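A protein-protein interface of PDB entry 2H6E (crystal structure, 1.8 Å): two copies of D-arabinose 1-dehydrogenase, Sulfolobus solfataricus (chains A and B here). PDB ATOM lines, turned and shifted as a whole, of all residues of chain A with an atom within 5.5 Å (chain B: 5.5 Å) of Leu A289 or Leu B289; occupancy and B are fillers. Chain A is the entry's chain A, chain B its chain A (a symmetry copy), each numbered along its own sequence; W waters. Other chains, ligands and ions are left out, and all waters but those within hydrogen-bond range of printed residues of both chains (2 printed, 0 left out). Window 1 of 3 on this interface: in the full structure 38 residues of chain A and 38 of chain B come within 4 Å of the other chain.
Val A275 touches Leu B277, and with the chains exchanged Leu A277 touches Val B275.
Thr A282 touches Leu B289, and with the chains exchanged Leu A289 touches Thr B282.
Lys A287 touches Gly B291, and with the chains exchanged Gly A291 touches Lys B287.
Leu A289 touches its own counterpart, Leu B289.
Of the 16 pairs that touch across the chains among the printed residues, 16 have their exchanged pair printed and touching as well.
Of the 12 printed residues of chain B, 8 touch a printed residue of chain A.
Hydrophobic or aromatic side chains of chain B that line the printed part of chain A: Val B275, Leu B277, Leu B289 and Leu B290.
Of the 12 printed residues of chain A, 8 touch a printed residue of chain B.
Among the printed residues, 16 pairs touch across the chains.
Among the printed residues, no Asp or Glu carboxylate lies within 4 Å of a Lys or Arg side-chain nitrogen of the other chain.
Thr A282 touches Leu B289 (CG2 to CD2, 3.7 Å).
Thr A282 touches Gly B291.
Lys A287 touches Leu B290.
Leu B289 touches Lys A288 (O to CA, 3.2 Å).
Leu B290 touches Lys A288 (CD2 to CG, 3.7 Å).
Thr B282 touches Leu A289.
Lys B288 touches Leu A289 (CA to O, 3.2 Å).
Leu A290 touches Lys B287 (C to O, 3.8 Å).
Lys B288 touches Leu A290.
CA of Gly A291 touches O of Thr B282, 3.6 Å away.
N of Leu A289 is in hydrogen-bond range of O of Leu B289, 2.8 Å away.
The backbone carbonyl oxygen (O) of Leu B277 sits at hydrogen-bond distance from the backbone NH (N) of Val A275 (2.8 Å).
N of Gly A291 lies within hydrogen-bond range of O of Lys B287 (2.8 Å).
The backbone carbonyl oxygen (O) of Leu A277 lies within hydrogen-bond range of the backbone NH (N) of Val B275, 2.8 Å away.
O of Lys A287 is in hydrogen-bond range of N of Gly B291 (2.8 Å).
Of the printed residues of chain B, Thr A282 touches Leu B289 (3.7 Å) and Gly B291 (3.6 Å).
Of chain B, only Thr B282 (3.7 Å), Lys B288 (3.2 Å) and Leu B289 (2.8 Å) come within 4 Å of Leu A289.
Printed residues of chain B within 4 Å of Leu A290: Lys B287, Lys B288 and Leu B290.
Printed residues of chain A within 4 Å of Leu B277: Val A275.
Of the printed residues of chain A, Lys B287 touches Leu A290 (3.8 Å) and Gly A291 (2.8 Å).
Of the printed residues of chain A, Lys B288 touches Leu A289 and Leu A290.
Of chain A, only Thr A282 (3.7 Å), Lys A288 (3.2 Å) and Leu A289 (2.8 Å) come within 4 Å of Leu B289.
The nearest residue of chain A that does not touch Leu B289 is Lys A287 (4.1 Å).
The nearest printed residue of chain B that does not touch Lys A287 is Leu B289 (4.1 Å).
Water W1 lies within hydrogen-bond range of the backbone carbonyl oxygen (O) of Gly A291 and the side-chain amino group (NZ) of Lys B288.
Water W2 lies within hydrogen-bond range of the backbone carbonyl oxygen (O) of Gly B291 and the side-chain amino group (NZ) of Lys A288.
The backbone carbonyl oxygen of Ile A265 is in hydrogen-bond range of the backbone NH of Leu A290, at 2.8 Å.
The backbone NH (N) of Leu B290 lies within hydrogen-bond range of the backbone carbonyl oxygen (O) of Ile B265, at 2.8 Å.
The backbone NH (N) of Ile A265 sits at hydrogen-bond distance from the backbone carbonyl oxygen (O) of Lys A288 (2.9 Å).
O of Thr B282 lies within hydrogen-bond range of N of Lys B287 (3.0 Å).
O of Thr A282 is in hydrogen-bond range of N of Lys A287, 3.0 Å away.
The backbone carbonyl oxygen (O) of Lys B288 sits at hydrogen-bond distance from the backbone NH (N) of Ile B265 (2.9 Å).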
ATOM      1  N   THR A 252      -5.011  -4.038 -22.650  1.00  0.00           N
ATOM      2  CA  THR A 252      -4.186  -2.828 -22.703  1.00  0.00           C
ATOM      3  C   THR A 252      -4.712  -1.832 -23.746  1.00  0.00           C
ATOM      4  O   THR A 252      -4.824  -0.635 -23.486  1.00  0.00           O
ATOM      5  CB  THR A 252      -2.711  -3.149 -22.965  1.00  0.00           C
ATOM      6  OG1 THR A 252      -2.569  -3.905 -24.170  1.00  0.00           O
ATOM      7  CG2 THR A 252      -2.101  -3.922 -21.754  1.00  0.00           C
ATOM      8  N   ALA A 264      -0.915   6.468 -17.491  1.00  0.00           N
ATOM      9  CA  ALA A 264      -0.168   5.241 -17.686  1.00  0.00           C
ATOM     10  C   ALA A 264      -0.978   4.012 -17.366  1.00  0.00           C
ATOM     11  O   ALA A 264      -1.798   4.003 -16.423  1.00  0.00           O
ATOM     12  CB  ALA A 264       1.128   5.230 -16.826  1.00  0.00           C
ATOM     13  N   ILE A 265      -0.717   2.969 -18.150  1.00  0.00           N
ATOM     14  CA  ILE A 265      -1.013   1.589 -17.756  1.00  0.00           C
ATOM     15  C   ILE A 265       0.210   1.029 -17.016  1.00  0.00           C
ATOM     16  O   ILE A 265       1.356   1.135 -17.482  1.00  0.00           O
ATOM     17  CB  ILE A 265      -1.300   0.680 -18.984  1.00  0.00           C
ATOM     18  CG1 ILE A 265      -2.473   1.206 -19.814  1.00  0.00           C
ATOM     19  CG2 ILE A 265      -1.520  -0.756 -18.534  1.00  0.00           C
ATOM     20  CD1 ILE A 265      -2.525   0.667 -21.225  1.00  0.00           C
ATOM     21  N   LEU A 267       1.488  -2.431 -16.295  1.00  0.00           N
ATOM     22  CA  LEU A 267       1.302  -3.781 -16.785  1.00  0.00           C
ATOM     23  C   LEU A 267       1.904  -4.794 -15.822  1.00  0.00           C
ATOM     24  O   LEU A 267       3.140  -4.969 -15.735  1.00  0.00           O
ATOM     25  CB  LEU A 267       1.923  -3.958 -18.184  1.00  0.00           C
ATOM     26  CG  LEU A 267       1.785  -5.359 -18.806  1.00  0.00           C
ATOM     27  CD1 LEU A 267       0.308  -5.630 -19.128  1.00  0.00           C
ATOM     28  CD2 LEU A 267       2.670  -5.522 -20.083  1.00  0.00           C
ATOM     29  N   VAL A 275       0.830  -7.448 -25.759  1.00  0.00           N
ATOM     30  CA  VAL A 275      -0.061  -6.358 -25.434  1.00  0.00           C
ATOM     31  C   VAL A 275      -0.075  -5.418 -26.639  1.00  0.00           C
ATOM     32  O   VAL A 275       0.824  -5.457 -27.487  1.00  0.00           O
ATOM     33  CB  VAL A 275       0.368  -5.647 -24.156  1.00  0.00           C
ATOM     34  CG1 VAL A 275       0.129  -6.577 -22.947  1.00  0.00           C
ATOM     35  CG2 VAL A 275       1.852  -5.178 -24.230  1.00  0.00           C
ATOM     36  N   LEU A 277      -1.554  -1.343 -28.192  1.00  0.00           N
ATOM     37  CA  LEU A 277      -2.069  -0.007 -27.954  1.00  0.00           C
ATOM     38  C   LEU A 277      -2.298   0.655 -29.301  1.00  0.00           C
ATOM     39  O   LEU A 277      -1.549   0.438 -30.253  1.00  0.00           O
ATOM     40  CB  LEU A 277      -1.075   0.841 -27.174  1.00  0.00           C
ATOM     41  CG  LEU A 277      -0.632   0.370 -25.790  1.00  0.00           C
ATOM     42  CD1 LEU A 277       0.587   1.178 -25.336  1.00  0.00           C
ATOM     43  CD2 LEU A 277      -1.764   0.475 -24.793  1.00  0.00           C
ATOM     44  N   THR A 282      -1.882   6.824 -28.193  1.00  0.00           N
ATOM     45  CA  THR A 282      -0.741   6.720 -27.295  1.00  0.00           C
ATOM     46  C   THR A 282       0.279   7.818 -27.571  1.00  0.00           C
ATOM     47  O   THR A 282       0.678   8.527 -26.655  1.00  0.00           O
ATOM     48  CB  THR A 282      -0.113   5.325 -27.362  1.00  0.00           C
ATOM     49  OG1 THR A 282      -1.147   4.352 -27.162  1.00  0.00           O
ATOM     50  CG2 THR A 282       0.980   5.147 -26.260  1.00  0.00           C
ATOM     51  N   LYS A 287       0.591   9.053 -23.731  1.00  0.00           N
ATOM     52  CA  LYS A 287       0.282   8.002 -22.800  1.00  0.00           C
ATOM     53  C   LYS A 287       1.411   6.991 -22.708  1.00  0.00           C
ATOM     54  O   LYS A 287       2.305   6.953 -23.560  1.00  0.00           O
ATOM     55  CB  LYS A 287      -1.023   7.349 -23.155  1.00  0.00           C
ATOM     56  CG  LYS A 287      -2.217   8.307 -23.102  1.00  0.00           C
ATOM     57  CD  LYS A 287      -3.506   7.626 -23.490  1.00  0.00           C
ATOM     58  CE  LYS A 287      -4.629   8.612 -23.497  1.00  0.00           C
ATOM     59  NZ  LYS A 287      -5.967   8.066 -23.899  1.00  0.00           N
ATOM     60  N   LYS A 288       1.356   6.161 -21.664  1.00  0.00           N
ATOM     61  CA  LYS A 288       2.486   5.332 -21.283  1.00  0.00           C
ATOM     62  C   LYS A 288       2.041   3.929 -20.927  1.00  0.00           C
ATOM     63  O   LYS A 288       0.930   3.725 -20.439  1.00  0.00           O
ATOM     64  CB  LYS A 288       3.184   5.907 -20.039  1.00  0.00           C
ATOM     65  CG  LYS A 288       3.622   7.351 -20.182  1.00  0.00           C
ATOM     66  CD  LYS A 288       3.961   8.009 -18.858  1.00  0.00           C
ATOM     67  CE  LYS A 288       4.456   9.430 -19.082  1.00  0.00           C
ATOM     68  NZ  LYS A 288       3.487  10.337 -19.755  1.00  0.00           N
ATOM     69  N   LEU A 289       2.944   2.982 -21.116  1.00  0.00           N
ATOM     70  CA  LEU A 289       2.776   1.641 -20.549  1.00  0.00           C
ATOM     71  C   LEU A 289       4.078   1.278 -19.834  1.00  0.00           C
ATOM     72  O   LEU A 289       5.156   1.355 -20.421  1.00  0.00           O
ATOM     73  CB  LEU A 289       2.391   0.618 -21.629  1.00  0.00           C
ATOM     74  CG  LEU A 289       2.157  -0.824 -21.153  1.00  0.00           C
ATOM     75  CD1 LEU A 289       1.153  -1.565 -22.016  1.00  0.00           C
ATOM     76  CD2 LEU A 289       3.526  -1.601 -21.109  1.00  0.00           C
ATOM     77  N   LEU A 290       3.958   0.922 -18.560  1.00  0.00           N
ATOM     78  CA  LEU A 290       5.087   0.652 -17.673  1.00  0.00           C
ATOM     79  C   LEU A 290       4.948  -0.776 -17.114  1.00  0.00           C
ATOM     80  O   LEU A 290       4.028  -1.064 -16.344  1.00  0.00           O
ATOM     81  CB  LEU A 290       5.060   1.667 -16.517  1.00  0.00           C
ATOM     82  CG  LEU A 290       4.882   3.145 -16.866  1.00  0.00           C
ATOM     83  CD1 LEU A 290       4.854   4.021 -15.584  1.00  0.00           C
ATOM     84  CD2 LEU A 290       6.002   3.579 -17.816  1.00  0.00           C
ATOM     85  N   GLY A 291       5.884  -1.646 -17.490  1.00  0.00           N
ATOM     86  CA  GLY A 291       5.957  -3.011 -16.997  1.00  0.00           C
ATOM     87  C   GLY A 291       6.275  -3.030 -15.522  1.00  0.00           C
ATOM     88  O   GLY A 291       7.090  -2.217 -15.056  1.00  0.00           O
ATOM     89  N   THR B 252       7.806  -1.594 -32.620  1.00  0.00           N
ATOM     90  CA  THR B 252       7.837  -1.534 -31.156  1.00  0.00           C
ATOM     91  C   THR B 252       8.105  -2.915 -30.541  1.00  0.00           C
ATOM     92  O   THR B 252       8.923  -3.062 -29.635  1.00  0.00           O
ATOM     93  CB  THR B 252       6.553  -0.929 -30.579  1.00  0.00           C
ATOM     94  OG1 THR B 252       5.410  -1.660 -31.026  1.00  0.00           O
ATOM     95  CG2 THR B 252       6.435   0.576 -30.977  1.00  0.00           C
ATOM     96  N   ALA B 264      13.232   2.034 -22.075  1.00  0.00           N
ATOM     97  CA  ALA B 264      12.012   2.561 -22.658  1.00  0.00           C
ATOM     98  C   ALA B 264      12.111   2.734 -24.151  1.00  0.00           C
ATOM     99  O   ALA B 264      13.175   3.105 -24.691  1.00  0.00           O
ATOM    100  CB  ALA B 264      11.627   3.924 -22.015  1.00  0.00           C
ATOM    101  N   ILE B 265      10.980   2.484 -24.804  1.00  0.00           N
ATOM    102  CA  ILE B 265      10.703   3.015 -26.141  1.00  0.00           C
ATOM    103  C   ILE B 265      10.025   4.383 -25.984  1.00  0.00           C
ATOM    104  O   ILE B 265       9.058   4.544 -25.221  1.00  0.00           O
ATOM    105  CB  ILE B 265       9.753   2.088 -26.954  1.00  0.00           C
ATOM    106  CG1 ILE B 265      10.332   0.679 -27.104  1.00  0.00           C
ATOM    107  CG2 ILE B 265       9.430   2.718 -28.299  1.00  0.00           C
ATOM    108  CD1 ILE B 265       9.312  -0.374 -27.464  1.00  0.00           C
ATOM    109  N   LEU B 267       7.844   6.505 -28.191  1.00  0.00           N
ATOM    110  CA  LEU B 267       7.019   6.353 -29.371  1.00  0.00           C
ATOM    111  C   LEU B 267       6.648   7.708 -29.952  1.00  0.00           C
ATOM    112  O   LEU B 267       5.790   8.445 -29.415  1.00  0.00           O
ATOM    113  CB  LEU B 267       5.741   5.553 -29.058  1.00  0.00           C
ATOM    114  CG  LEU B 267       4.783   5.328 -30.242  1.00  0.00           C
ATOM    115  CD1 LEU B 267       5.446   4.390 -31.262  1.00  0.00           C
ATOM    116  CD2 LEU B 267       3.404   4.757 -29.780  1.00  0.00           C
ATOM    117  N   VAL B 275       0.498  -0.364 -31.932  1.00  0.00           N
ATOM    118  CA  VAL B 275       1.814  -0.821 -31.555  1.00  0.00           C
ATOM    119  C   VAL B 275       1.624  -2.064 -30.687  1.00  0.00           C
ATOM    120  O   VAL B 275       0.536  -2.305 -30.150  1.00  0.00           O
ATOM    121  CB  VAL B 275       2.598   0.268 -30.833  1.00  0.00           C
ATOM    122  CG1 VAL B 275       2.963   1.386 -31.833  1.00  0.00           C
ATOM    123  CG2 VAL B 275       1.809   0.831 -29.612  1.00  0.00           C
ATOM    124  N   LEU B 277       3.780  -5.133 -28.016  1.00  0.00           N
ATOM    125  CA  LEU B 277       4.925  -5.535 -27.217  1.00  0.00           C
ATOM    126  C   LEU B 277       4.658  -6.934 -26.688  1.00  0.00           C
ATOM    127  O   LEU B 277       3.522  -7.290 -26.373  1.00  0.00           O
ATOM    128  CB  LEU B 277       5.126  -4.610 -26.026  1.00  0.00           C
ATOM    129  CG  LEU B 277       5.367  -3.123 -26.282  1.00  0.00           C
ATOM    130  CD1 LEU B 277       5.216  -2.345 -24.972  1.00  0.00           C
ATOM    131  CD2 LEU B 277       6.724  -2.893 -26.906  1.00  0.00           C
ATOM    132  N   THR B 282       8.091  -7.388 -21.447  1.00  0.00           N
ATOM    133  CA  THR B 282       7.782  -6.048 -20.970  1.00  0.00           C
ATOM    134  C   THR B 282       7.504  -6.046 -19.473  1.00  0.00           C
ATOM    135  O   THR B 282       8.104  -5.271 -18.740  1.00  0.00           O
ATOM    136  CB  THR B 282       6.631  -5.431 -21.769  1.00  0.00           C
ATOM    137  OG1 THR B 282       6.938  -5.535 -23.165  1.00  0.00           O
ATOM    138  CG2 THR B 282       6.430  -3.928 -21.397  1.00  0.00           C
ATOM    139  N   LYS B 287      10.053  -3.031 -18.591  1.00  0.00           N
ATOM    140  CA  LYS B 287      10.251  -2.147 -19.708  1.00  0.00           C
ATOM    141  C   LYS B 287       9.046  -1.247 -19.923  1.00  0.00           C
ATOM    142  O   LYS B 287       7.961  -1.494 -19.387  1.00  0.00           O
ATOM    143  CB  LYS B 287      10.591  -2.928 -20.947  1.00  0.00           C
ATOM    144  CG  LYS B 287      11.890  -3.728 -20.823  1.00  0.00           C
ATOM    145  CD  LYS B 287      12.187  -4.520 -22.072  1.00  0.00           C
ATOM    146  CE  LYS B 287      13.421  -5.341 -21.881  1.00  0.00           C
ATOM    147  NZ  LYS B 287      13.810  -6.204 -23.045  1.00  0.00           N
ATOM    148  N   LYS B 288       9.250  -0.199 -20.724  1.00  0.00           N
ATOM    149  CA  LYS B 288       8.298   0.895 -20.812  1.00  0.00           C
ATOM    150  C   LYS B 288       8.086   1.325 -22.249  1.00  0.00           C
ATOM    151  O   LYS B 288       8.992   1.224 -23.076  1.00  0.00           O
ATOM    152  CB  LYS B 288       8.815   2.125 -20.050  1.00  0.00           C
ATOM    153  CG  LYS B 288       9.169   1.857 -18.600  1.00  0.00           C
ATOM    154  CD  LYS B 288      10.011   2.952 -17.976  1.00  0.00           C
ATOM    155  CE  LYS B 288      10.271   2.652 -16.507  1.00  0.00           C
ATOM    156  NZ  LYS B 288      10.993   1.378 -16.243  1.00  0.00           N
ATOM    157  N   LEU B 289       6.910   1.863 -22.512  1.00  0.00           N
ATOM    158  CA  LEU B 289       6.664   2.591 -23.761  1.00  0.00           C
ATOM    159  C   LEU B 289       6.017   3.927 -23.395  1.00  0.00           C
ATOM    160  O   LEU B 289       5.016   3.963 -22.683  1.00  0.00           O
ATOM    161  CB  LEU B 289       5.805   1.767 -24.733  1.00  0.00           C
ATOM    162  CG  LEU B 289       5.502   2.413 -26.094  1.00  0.00           C
ATOM    163  CD1 LEU B 289       5.315   1.386 -27.195  1.00  0.00           C
ATOM    164  CD2 LEU B 289       4.230   3.334 -25.979  1.00  0.00           C
ATOM    165  N   LEU B 290       6.628   5.012 -23.859  1.00  0.00           N
ATOM    166  CA  LEU B 290       6.239   6.379 -23.528  1.00  0.00           C
ATOM    167  C   LEU B 290       5.926   7.138 -24.830  1.00  0.00           C
ATOM    168  O   LEU B 290       6.821   7.388 -25.642  1.00  0.00           O
ATOM    169  CB  LEU B 290       7.409   7.062 -22.798  1.00  0.00           C
ATOM    170  CG  LEU B 290       8.073   6.306 -21.646  1.00  0.00           C
ATOM    171  CD1 LEU B 290       9.245   7.128 -21.041  1.00  0.00           C
ATOM    172  CD2 LEU B 290       7.019   5.971 -20.586  1.00  0.00           C
ATOM    173  N   GLY B 291       4.660   7.519 -24.997  1.00  0.00           N
ATOM    174  CA  GLY B 291       4.204   8.313 -26.125  1.00  0.00           C
ATOM    175  C   GLY B 291       4.805   9.696 -26.084  1.00  0.00           C
ATOM    176  O   GLY B 291       4.931  10.282 -24.997  1.00  0.00           O
HETATM  177  O   HOH W   1       8.436   0.119 -15.511  1.00  0.00           O
HETATM  178  O   HOH W   2       4.958   9.982 -22.279  1.00  0.00           O
